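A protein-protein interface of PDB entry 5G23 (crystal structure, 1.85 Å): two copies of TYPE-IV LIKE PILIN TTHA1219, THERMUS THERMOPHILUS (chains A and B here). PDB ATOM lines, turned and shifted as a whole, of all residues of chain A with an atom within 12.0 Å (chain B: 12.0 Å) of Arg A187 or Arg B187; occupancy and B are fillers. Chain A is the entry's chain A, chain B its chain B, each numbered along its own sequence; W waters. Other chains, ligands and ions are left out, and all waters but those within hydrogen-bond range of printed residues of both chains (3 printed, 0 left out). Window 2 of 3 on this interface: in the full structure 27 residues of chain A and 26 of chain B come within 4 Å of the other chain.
Arg B44 touches its own counterpart, Arg A44.
Arg A44 touches Glu B139, and with the chains exchanged Glu A139 touches Arg B44.
Arg A44 touches Val B184, and with the chains exchanged Val A184 touches Arg B44.
Arg B187 touches its own counterpart, Arg A187.
16 positions are printed for both chains.
Of the 6 pairs that touch across the chains among the printed residues, 6 have their exchanged pair printed and touching as well.
Of the 16 printed residues of chain B, 4 touch a printed residue of chain A.
Printed residues of chain B that touch a printed residue of chain A: Arg B44, Glu B139, Val B184 and Arg B187.
Of the 17 printed residues of chain A, 4 touch a printed residue of chain B.
Hydrophobic or aromatic side chains of chain A within 4 Å of the printed part of chain B: Val A184.
The guanidinium group (NH1) of Arg A187 lies close to the guanidinium group (NE) of Arg B187 (3.1 Å).
The side-chain carboxylate (OE2) of Glu B139 lies within salt-bridge range of the guanidinium group (NH1) of Arg A44, at 2.8 Å.
The side-chain carboxylate (OE2) of Glu A139 is in salt-bridge range of the guanidinium group (NH1) of Arg B44.
Printed residues of chain B within 4 Å of Glu A139: Arg B44 (2.7 Å).
Of the printed residues of chain B, Val A184 touches Arg B44.
No residue of chain B comes within 4 Å of Pro A185.
No residue of chain B comes within 4 Å of Val A186.
Of chain B, only Arg B187 (3.1 Å) comes within 4 Å of Arg A187.
No residue of chain B comes within 4 Å of Gly A188.
No residue of chain B comes within 4 Å of Gly A189.
No residue of chain A comes within 4 Å of Pro B185.
Arg B187 touches just one residue of chain A: Arg A187 (3.1 Å).
No residue of chain A comes within 4 Å of Gly B188.
No residue of chain A comes within 4 Å of Gly B189.
Ala B190 touches none of the printed residues of chain A.
The nearest residue of chain B that does not touch Arg A187 is Glu B139 (8.3 Å).
The nearest residue of chain A that does not touch Arg B187 is Gly A188 (8.4 Å).
The nearest printed residue of chain B that does not touch Val A184 is Glu B139 (7.1 Å).
Among the printed residues, merely in contact across the chains: Arg A44 with Arg B44 (3.4 Å), Arg A44 with Val B184 (3.7 Å) and Val A184 with Arg B44 (3.7 Å).
Water W1 bridges the backbone carbonyl oxygen (O) of Pro B185 (2.8 Å) and the guanidinium group (NH1) of Arg A44 (3.3 Å).
Water W2 bridges OE1 of Glu A139 (2.9 Å) and N of Arg B44 (3.0 Å).
Water W3 bridges NH2 of Arg B187 (3.2 Å) and NH2 of Arg A187 (3.4 Å).
The backbone carbonyl oxygen of Glu A139 lies within hydrogen-bond range of the guanidinium group of Arg A220 (3.0 Å).
NH2 of Arg B220 sits at hydrogen-bond distance from O of Glu B139, at 3.0 Å.
The backbone NH (N) of Leu B221 lies within hydrogen-bond range of the backbone carbonyl oxygen (O) of Val B184 (2.8 Å).
O of Val A184 sits at hydrogen-bond distance from N of Leu A221, at 2.8 Å.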
ATOM      1  N   ARG A  44     -20.340   4.073  -9.827  1.00  0.00           N
ATOM      2  CA  ARG A  44     -21.469   3.419  -9.267  1.00  0.00           C
ATOM      3  C   ARG A  44     -21.191   2.827  -7.875  1.00  0.00           C
ATOM      4  O   ARG A  44     -22.003   2.963  -6.949  1.00  0.00           O
ATOM      5  CB  ARG A  44     -21.887   2.308 -10.226  1.00  0.00           C
ATOM      6  CG  ARG A  44     -23.057   1.516  -9.774  1.00  0.00           C
ATOM      7  CD  ARG A  44     -23.426   0.429 -10.779  1.00  0.00           C
ATOM      8  NE  ARG A  44     -24.473  -0.429 -10.271  1.00  0.00           N
ATOM      9  CZ  ARG A  44     -24.924  -1.502 -10.875  1.00  0.00           C
ATOM     10  NH1 ARG A  44     -24.378  -1.862 -11.987  1.00  0.00           N
ATOM     11  NH2 ARG A  44     -25.903  -2.229 -10.360  1.00  0.00           N
ATOM     12  N   LEU A  45     -20.044   2.157  -7.723  1.00  0.00           N
ATOM     13  CA  LEU A  45     -19.699   1.544  -6.432  1.00  0.00           C
ATOM     14  C   LEU A  45     -19.434   2.644  -5.374  1.00  0.00           C
ATOM     15  O   LEU A  45     -19.888   2.533  -4.238  1.00  0.00           O
ATOM     16  CB  LEU A  45     -18.480   0.595  -6.572  1.00  0.00           C
ATOM     17  CG  LEU A  45     -18.107  -0.130  -5.307  1.00  0.00           C
ATOM     18  CD1 LEU A  45     -19.270  -0.927  -4.759  1.00  0.00           C
ATOM     19  CD2 LEU A  45     -16.966  -1.105  -5.575  1.00  0.00           C
ATOM     20  N   GLU A 139     -22.999  -9.694  -6.092  1.00  0.00           N
ATOM     21  CA  GLU A 139     -22.073  -9.063  -7.053  1.00  0.00           C
ATOM     22  C   GLU A 139     -21.080  -8.151  -6.289  1.00  0.00           C
ATOM     23  O   GLU A 139     -19.865  -8.222  -6.454  1.00  0.00           O
ATOM     24  CB  GLU A 139     -22.937  -8.311  -8.119  1.00  0.00           C
ATOM     25  CG  GLU A 139     -22.218  -7.564  -9.226  1.00  0.00           C
ATOM     26  CD  GLU A 139     -23.206  -6.746 -10.138  1.00  0.00           C
ATOM     27  OE1 GLU A 139     -24.390  -7.101 -10.202  1.00  0.00           O
ATOM     28  OE2 GLU A 139     -22.827  -5.750 -10.778  1.00  0.00           O
ATOM     29  N   SER A 183     -15.726  -4.575  -3.342  1.00  0.00           N
ATOM     30  CA  SER A 183     -15.331  -4.929  -4.666  1.00  0.00           C
ATOM     31  C   SER A 183     -16.483  -5.476  -5.490  1.00  0.00           C
ATOM     32  O   SER A 183     -17.428  -6.045  -4.979  1.00  0.00           O
ATOM     33  CB  SER A 183     -14.185  -5.999  -4.649  1.00  0.00           C
ATOM     34  OG  SER A 183     -14.656  -7.281  -4.242  1.00  0.00           O
ATOM     35  N   VAL A 184     -16.335  -5.338  -6.805  1.00  0.00           N
ATOM     36  CA  VAL A 184     -17.278  -5.853  -7.789  1.00  0.00           C
ATOM     37  C   VAL A 184     -16.526  -6.290  -9.046  1.00  0.00           C
ATOM     38  O   VAL A 184     -15.461  -5.726  -9.366  1.00  0.00           O
ATOM     39  CB  VAL A 184     -18.285  -4.779  -8.288  1.00  0.00           C
ATOM     40  CG1 VAL A 184     -19.279  -4.392  -7.244  1.00  0.00           C
ATOM     41  CG2 VAL A 184     -17.595  -3.525  -8.811  1.00  0.00           C
ATOM     42  N   PRO A 185     -17.079  -7.256  -9.786  1.00  0.00           N
ATOM     43  CA  PRO A 185     -16.470  -7.620 -11.055  1.00  0.00           C
ATOM     44  C   PRO A 185     -16.684  -6.523 -12.076  1.00  0.00           C
ATOM     45  O   PRO A 185     -17.645  -5.783 -11.969  1.00  0.00           O
ATOM     46  CB  PRO A 185     -17.253  -8.846 -11.521  1.00  0.00           C
ATOM     47  CG  PRO A 185     -18.125  -9.222 -10.428  1.00  0.00           C
ATOM     48  CD  PRO A 185     -18.299  -8.042  -9.518  1.00  0.00           C
ATOM     49  N   VAL A 186     -15.763  -6.406 -13.035  1.00  0.00           N
ATOM     50  CA  VAL A 186     -15.904  -5.377 -14.091  1.00  0.00           C
ATOM     51  C   VAL A 186     -15.316  -5.959 -15.368  1.00  0.00           C
ATOM     52  O   VAL A 186     -14.261  -6.577 -15.351  1.00  0.00           O
ATOM     53  CB  VAL A 186     -15.255  -4.019 -13.671  1.00  0.00           C
ATOM     54  CG1 VAL A 186     -13.749  -4.121 -13.548  1.00  0.00           C
ATOM     55  CG2 VAL A 186     -15.626  -2.919 -14.654  1.00  0.00           C
ATOM     56  N   ARG A 187     -16.025  -5.776 -16.472  1.00  0.00           N
ATOM     57  CA  ARG A 187     -15.604  -6.296 -17.752  1.00  0.00           C
ATOM     58  C   ARG A 187     -14.240  -5.702 -18.111  1.00  0.00           C
ATOM     59  O   ARG A 187     -14.100  -4.493 -18.099  1.00  0.00           O
ATOM     60  CB  ARG A 187     -16.647  -5.920 -18.817  1.00  0.00           C
ATOM     61  CG  ARG A 187     -16.196  -6.166 -20.297  1.00  0.00           C
ATOM     62  CD  ARG A 187     -16.634  -7.518 -20.828  1.00  0.00           C
ATOM     63  NE  ARG A 187     -16.251  -7.808 -22.236  1.00  0.00           N
ATOM     64  CZ  ARG A 187     -16.523  -8.968 -22.834  1.00  0.00           C
ATOM     65  NH1 ARG A 187     -17.164  -9.918 -22.169  1.00  0.00           N
ATOM     66  NH2 ARG A 187     -16.146  -9.187 -24.078  1.00  0.00           N
ATOM     67  N   GLY A 188     -13.248  -6.556 -18.367  1.00  0.00           N
ATOM     68  CA  GLY A 188     -11.912  -6.107 -18.749  1.00  0.00           C
ATOM     69  C   GLY A 188     -10.974  -5.970 -17.560  1.00  0.00           C
ATOM     70  O   GLY A 188      -9.762  -5.802 -17.731  1.00  0.00           O
ATOM     71  N   GLY A 189     -11.504  -6.092 -16.351  1.00  0.00           N
ATOM     72  CA  GLY A 189     -10.676  -6.045 -15.159  1.00  0.00           C
ATOM     73  C   GLY A 189     -10.311  -4.638 -14.710  1.00  0.00           C
ATOM     74  O   GLY A 189     -10.520  -3.666 -15.417  1.00  0.00           O
ATOM     75  N   ALA A 190      -9.799  -4.526 -13.502  1.00  0.00           N
ATOM     76  CA  ALA A 190      -9.350  -3.247 -12.958  1.00  0.00           C
ATOM     77  C   ALA A 190      -7.985  -3.454 -12.404  1.00  0.00           C
ATOM     78  O   ALA A 190      -7.611  -4.581 -12.105  1.00  0.00           O
ATOM     79  CB  ALA A 190     -10.264  -2.827 -11.843  1.00  0.00           C
ATOM     80  N   PRO A 191      -7.235  -2.370 -12.215  1.00  0.00           N
ATOM     81  CA  PRO A 191      -5.895  -2.574 -11.724  1.00  0.00           C
ATOM     82  C   PRO A 191      -5.921  -2.880 -10.239  1.00  0.00           C
ATOM     83  O   PRO A 191      -6.932  -2.665  -9.598  1.00  0.00           O
ATOM     84  CB  PRO A 191      -5.174  -1.236 -12.017  1.00  0.00           C
ATOM     85  CG  PRO A 191      -6.221  -0.257 -12.320  1.00  0.00           C
ATOM     86  CD  PRO A 191      -7.483  -0.996 -12.686  1.00  0.00           C
ATOM     87  N   ASP A 218      -6.970  -9.615  -8.129  1.00  0.00           N
ATOM     88  CA  ASP A 218      -7.943 -10.517  -8.736  1.00  0.00           C
ATOM     89  C   ASP A 218      -8.722  -9.866  -9.867  1.00  0.00           C
ATOM     90  O   ASP A 218      -9.678 -10.454 -10.368  1.00  0.00           O
ATOM     91  CB  ASP A 218      -8.925 -11.060  -7.686  1.00  0.00           C
ATOM     92  CG  ASP A 218      -9.703  -9.955  -6.978  1.00  0.00           C
ATOM     93  OD1 ASP A 218      -9.594  -8.770  -7.387  1.00  0.00           O
ATOM     94  OD2 ASP A 218     -10.389 -10.263  -5.972  1.00  0.00           O
ATOM     95  N   GLY A 219      -8.327  -8.657 -10.252  1.00  0.00           N
ATOM     96  CA  GLY A 219      -8.932  -7.948 -11.354  1.00  0.00           C
ATOM     97  C   GLY A 219     -10.300  -7.322 -11.033  1.00  0.00           C
ATOM     98  O   GLY A 219     -10.951  -6.766 -11.943  1.00  0.00           O
ATOM     99  N   ARG A 220     -10.763  -7.442  -9.774  1.00  0.00           N
ATOM    100  CA  ARG A 220     -12.042  -6.825  -9.410  1.00  0.00           C
ATOM    101  C   ARG A 220     -11.864  -5.348  -9.199  1.00  0.00           C
ATOM    102  O   ARG A 220     -10.796  -4.878  -8.794  1.00  0.00           O
ATOM    103  CB  ARG A 220     -12.646  -7.476  -8.167  1.00  0.00           C
ATOM    104  CG  ARG A 220     -13.129  -8.889  -8.445  1.00  0.00           C
ATOM    105  CD  ARG A 220     -13.507  -9.609  -7.125  1.00  0.00           C
ATOM    106  NE  ARG A 220     -14.678  -9.073  -6.454  1.00  0.00           N
ATOM    107  CZ  ARG A 220     -15.951  -9.422  -6.685  1.00  0.00           C
ATOM    108  NH1 ARG A 220     -16.269 -10.366  -7.542  1.00  0.00           N
ATOM    109  NH2 ARG A 220     -16.933  -8.823  -6.055  1.00  0.00           N
ATOM    110  N   LEU A 221     -12.918  -4.602  -9.479  1.00  0.00           N
ATOM    111  CA  LEU A 221     -12.902  -3.158  -9.182  1.00  0.00           C
ATOM    112  C   LEU A 221     -13.107  -2.953  -7.698  1.00  0.00           C
ATOM    113  O   LEU A 221     -14.051  -3.525  -7.151  1.00  0.00           O
ATOM    114  CB  LEU A 221     -14.019  -2.497  -9.975  1.00  0.00           C
ATOM    115  CG  LEU A 221     -14.264  -1.026  -9.754  1.00  0.00           C
ATOM    116  CD1 LEU A 221     -13.022  -0.265 -10.082  1.00  0.00           C
ATOM    117  CD2 LEU A 221     -15.393  -0.458 -10.617  1.00  0.00           C
ATOM    118  N   ARG A 222     -12.247  -2.189  -7.058  1.00  0.00           N
ATOM    119  CA  ARG A 222     -12.366  -1.891  -5.654  1.00  0.00           C
ATOM    120  C   ARG A 222     -12.581  -0.409  -5.397  1.00  0.00           C
ATOM    121  O   ARG A 222     -12.022   0.450  -6.082  1.00  0.00           O
ATOM    122  CB  ARG A 222     -11.163  -2.362  -4.818  1.00  0.00           C
ATOM    123  CG  ARG A 222     -11.273  -3.814  -4.511  1.00  0.00           C
ATOM    124  CD  ARG A 222     -10.077  -4.400  -3.788  1.00  0.00           C
ATOM    125  NE  ARG A 222     -10.448  -5.781  -3.602  1.00  0.00           N
ATOM    126  CZ  ARG A 222     -10.339  -6.749  -4.510  1.00  0.00           C
ATOM    127  NH1 ARG A 222      -9.728  -6.571  -5.661  1.00  0.00           N
ATOM    128  NH2 ARG A 222     -10.838  -7.929  -4.245  1.00  0.00           N
ATOM    129  N   ARG B  44     -28.303  -6.186  -7.082  1.00  0.00           N
ATOM    130  CA  ARG B  44     -27.488  -5.059  -6.751  1.00  0.00           C
ATOM    131  C   ARG B  44     -28.205  -3.695  -6.885  1.00  0.00           C
ATOM    132  O   ARG B  44     -28.153  -2.846  -5.987  1.00  0.00           O
ATOM    133  CB  ARG B  44     -26.212  -5.110  -7.606  1.00  0.00           C
ATOM    134  CG  ARG B  44     -25.259  -3.999  -7.340  1.00  0.00           C
ATOM    135  CD  ARG B  44     -24.022  -4.084  -8.222  1.00  0.00           C
ATOM    136  NE  ARG B  44     -23.159  -2.945  -8.028  1.00  0.00           N
ATOM    137  CZ  ARG B  44     -22.154  -2.627  -8.814  1.00  0.00           C
ATOM    138  NH1 ARG B  44     -21.857  -3.411  -9.820  1.00  0.00           N
ATOM    139  NH2 ARG B  44     -21.398  -1.576  -8.564  1.00  0.00           N
ATOM    140  N   GLU B 139     -23.231   4.817 -14.998  1.00  0.00           N
ATOM    141  CA  GLU B 139     -23.649   3.481 -15.328  1.00  0.00           C
ATOM    142  C   GLU B 139     -25.137   3.377 -14.937  1.00  0.00           C
ATOM    143  O   GLU B 139     -25.952   2.815 -15.688  1.00  0.00           O
ATOM    144  CB  GLU B 139     -22.687   2.491 -14.561  1.00  0.00           C
ATOM    145  CG  GLU B 139     -22.923   1.012 -14.746  1.00  0.00           C
ATOM    146  CD  GLU B 139     -21.958   0.131 -13.914  1.00  0.00           C
ATOM    147  OE1 GLU B 139     -20.841   0.611 -13.591  1.00  0.00           O
ATOM    148  OE2 GLU B 139     -22.286  -1.057 -13.605  1.00  0.00           O
ATOM    149  N   SER B 183     -32.066   2.157 -14.328  1.00  0.00           N
ATOM    150  CA  SER B 183     -31.514   1.115 -15.216  1.00  0.00           C
ATOM    151  C   SER B 183     -30.022   1.075 -15.178  1.00  0.00           C
ATOM    152  O   SER B 183     -29.337   2.075 -14.923  1.00  0.00           O
ATOM    153  CB  SER B 183     -31.974   1.337 -16.678  1.00  0.00           C
ATOM    154  OG  SER B 183     -31.347   2.485 -17.279  1.00  0.00           O
ATOM    155  N   VAL B 184     -29.521  -0.094 -15.525  1.00  0.00           N
ATOM    156  CA  VAL B 184     -28.076  -0.322 -15.677  1.00  0.00           C
ATOM    157  C   VAL B 184     -27.830  -1.353 -16.766  1.00  0.00           C
ATOM    158  O   VAL B 184     -28.687  -2.237 -17.012  1.00  0.00           O
ATOM    159  CB  VAL B 184     -27.416  -0.935 -14.377  1.00  0.00           C
ATOM    160  CG1 VAL B 184     -27.323   0.040 -13.250  1.00  0.00           C
ATOM    161  CG2 VAL B 184     -28.097  -2.200 -13.936  1.00  0.00           C
ATOM    162  N   PRO B 185     -26.660  -1.303 -17.401  1.00  0.00           N
ATOM    163  CA  PRO B 185     -26.322  -2.363 -18.374  1.00  0.00           C
ATOM    164  C   PRO B 185     -26.088  -3.694 -17.703  1.00  0.00           C
ATOM    165  O   PRO B 185     -25.636  -3.707 -16.556  1.00  0.00           O
ATOM    166  CB  PRO B 185     -25.018  -1.892 -19.007  1.00  0.00           C
ATOM    167  CG  PRO B 185     -24.784  -0.512 -18.536  1.00  0.00           C
ATOM    168  CD  PRO B 185     -25.579  -0.315 -17.264  1.00  0.00           C
ATOM    169  N   VAL B 186     -26.375  -4.768 -18.416  1.00  0.00           N
ATOM    170  CA  VAL B 186     -26.079  -6.124 -17.956  1.00  0.00           C
ATOM    171  C   VAL B 186     -25.709  -6.968 -19.170  1.00  0.00           C
ATOM    172  O   VAL B 186     -26.370  -6.930 -20.202  1.00  0.00           O
ATOM    173  CB  VAL B 186     -27.266  -6.693 -17.122  1.00  0.00           C
ATOM    174  CG1 VAL B 186     -28.482  -6.972 -17.990  1.00  0.00           C
ATOM    175  CG2 VAL B 186     -26.844  -7.982 -16.396  1.00  0.00           C
ATOM    176  N   ARG B 187     -24.630  -7.735 -19.054  1.00  0.00           N
ATOM    177  CA  ARG B 187     -24.130  -8.529 -20.202  1.00  0.00           C
ATOM    178  C   ARG B 187     -25.200  -9.545 -20.593  1.00  0.00           C
ATOM    179  O   ARG B 187     -25.761 -10.227 -19.737  1.00  0.00           O
ATOM    180  CB  ARG B 187     -22.805  -9.244 -19.943  1.00  0.00           C
ATOM    181  CG  ARG B 187     -22.080  -9.620 -21.268  1.00  0.00           C
ATOM    182  CD  ARG B 187     -20.563  -9.780 -21.376  1.00  0.00           C
ATOM    183  NE  ARG B 187     -20.178 -10.048 -22.784  1.00  0.00           N
ATOM    184  CZ  ARG B 187     -19.837  -9.142 -23.718  1.00  0.00           C
ATOM    185  NH1 ARG B 187     -19.790  -7.843 -23.442  1.00  0.00           N
ATOM    186  NH2 ARG B 187     -19.522  -9.543 -24.931  1.00  0.00           N
ATOM    187  N   GLY B 188     -25.583  -9.521 -21.851  1.00  0.00           N
ATOM    188  CA  GLY B 188     -26.623 -10.434 -22.381  1.00  0.00           C
ATOM    189  C   GLY B 188     -28.015  -9.833 -22.374  1.00  0.00           C
ATOM    190  O   GLY B 188     -28.933 -10.370 -23.004  1.00  0.00           O
ATOM    191  N   GLY B 189     -28.179  -8.711 -21.684  1.00  0.00           N
ATOM    192  CA  GLY B 189     -29.451  -8.018 -21.679  1.00  0.00           C
ATOM    193  C   GLY B 189     -30.402  -8.576 -20.674  1.00  0.00           C
ATOM    194  O   GLY B 189     -30.181  -9.652 -20.096  1.00  0.00           O
ATOM    195  N   ALA B 190     -31.484  -7.846 -20.451  1.00  0.00           N
ATOM    196  CA  ALA B 190     -32.555  -8.279 -19.554  1.00  0.00           C
ATOM    197  C   ALA B 190     -33.830  -8.195 -20.315  1.00  0.00           C
ATOM    198  O   ALA B 190     -33.972  -7.414 -21.268  1.00  0.00           O
ATOM    199  CB  ALA B 190     -32.588  -7.370 -18.347  1.00  0.00           C
ATOM    200  N   PRO B 191     -34.798  -8.998 -19.938  1.00  0.00           N
ATOM    201  CA  PRO B 191     -36.075  -8.855 -20.620  1.00  0.00           C
ATOM    202  C   PRO B 191     -36.726  -7.498 -20.381  1.00  0.00           C
ATOM    203  O   PRO B 191     -36.466  -6.843 -19.372  1.00  0.00           O
ATOM    204  CB  PRO B 191     -36.922 -10.015 -20.075  1.00  0.00           C
ATOM    205  CG  PRO B 191     -36.227 -10.504 -18.846  1.00  0.00           C
ATOM    206  CD  PRO B 191     -34.817  -9.956 -18.826  1.00  0.00           C
ATOM    207  N   ASP B 218     -33.906  -1.195 -24.901  1.00  0.00           N
ATOM    208  CA  ASP B 218     -32.472  -1.102 -24.985  1.00  0.00           C
ATOM    209  C   ASP B 218     -31.766  -2.240 -24.246  1.00  0.00           C
ATOM    210  O   ASP B 218     -30.516  -2.194 -24.153  1.00  0.00           O
ATOM    211  CB  ASP B 218     -32.036   0.203 -24.413  1.00  0.00           C
ATOM    212  CG  ASP B 218     -32.443   0.367 -22.955  1.00  0.00           C
ATOM    213  OD1 ASP B 218     -32.891  -0.643 -22.272  1.00  0.00           O
ATOM    214  OD2 ASP B 218     -32.430   1.510 -22.488  1.00  0.00           O
ATOM    215  N   GLY B 219     -32.506  -3.283 -23.827  1.00  0.00           N
ATOM    216  CA  GLY B 219     -31.883  -4.462 -23.207  1.00  0.00           C
ATOM    217  C   GLY B 219     -31.357  -4.225 -21.774  1.00  0.00           C
ATOM    218  O   GLY B 219     -30.820  -5.124 -21.134  1.00  0.00           O
ATOM    219  N   ARG B 220     -31.443  -3.005 -21.248  1.00  0.00           N
ATOM    220  CA  ARG B 220     -30.875  -2.725 -19.893  1.00  0.00           C
ATOM    221  C   ARG B 220     -31.659  -3.396 -18.777  1.00  0.00           C
ATOM    222  O   ARG B 220     -32.877  -3.652 -18.904  1.00  0.00           O
ATOM    223  CB  ARG B 220     -30.795  -1.231 -19.665  1.00  0.00           C
ATOM    224  CG  ARG B 220     -29.707  -0.594 -20.506  1.00  0.00           C
ATOM    225  CD  ARG B 220     -29.790   0.895 -20.486  1.00  0.00           C
ATOM    226  NE  ARG B 220     -29.450   1.481 -19.211  1.00  0.00           N
ATOM    227  CZ  ARG B 220     -28.272   2.006 -18.868  1.00  0.00           C
ATOM    228  NH1 ARG B 220     -27.231   1.880 -19.624  1.00  0.00           N
ATOM    229  NH2 ARG B 220     -28.137   2.597 -17.702  1.00  0.00           N
ATOM    230  N   LEU B 221     -30.978  -3.693 -17.679  1.00  0.00           N
ATOM    231  CA  LEU B 221     -31.664  -4.177 -16.478  1.00  0.00           C
ATOM    232  C   LEU B 221     -32.352  -2.993 -15.799  1.00  0.00           C
ATOM    233  O   LEU B 221     -31.701  -1.985 -15.540  1.00  0.00           O
ATOM    234  CB  LEU B 221     -30.658  -4.787 -15.511  1.00  0.00           C
ATOM    235  CG  LEU B 221     -31.118  -5.448 -14.222  1.00  0.00           C
ATOM    236  CD1 LEU B 221     -30.112  -6.440 -13.669  1.00  0.00           C
ATOM    237  CD2 LEU B 221     -31.235  -4.370 -13.180  1.00  0.00           C
ATOM    238  N   ARG B 222     -33.619  -3.162 -15.467  1.00  0.00           N
ATOM    239  CA  ARG B 222     -34.406  -2.137 -14.790  1.00  0.00           C
ATOM    240  C   ARG B 222     -34.921  -2.614 -13.463  1.00  0.00           C
ATOM    241  O   ARG B 222     -35.225  -3.808 -13.301  1.00  0.00           O
ATOM    242  CB  ARG B 222     -35.551  -1.650 -15.633  1.00  0.00           C
ATOM    243  CG  ARG B 222     -35.102  -0.661 -16.667  1.00  0.00           C
ATOM    244  CD  ARG B 222     -36.197  -0.159 -17.618  1.00  0.00           C
ATOM    245  NE  ARG B 222     -35.496   0.847 -18.436  1.00  0.00           N
ATOM    246  CZ  ARG B 222     -34.697   0.597 -19.481  1.00  0.00           C
ATOM    247  NH1 ARG B 222     -34.692  -0.582 -20.101  1.00  0.00           N
ATOM    248  NH2 ARG B 222     -33.958   1.572 -19.991  1.00  0.00           N
HETATM  249  O   HOH W   1     -25.076  -4.407 -13.931  1.00  0.00           O
HETATM  250  O   HOH W   2     -26.779  -8.047  -8.858  1.00  0.00           O
HETATM  251  O   HOH W   3     -17.418  -8.633 -27.220  1.00  0.00           O
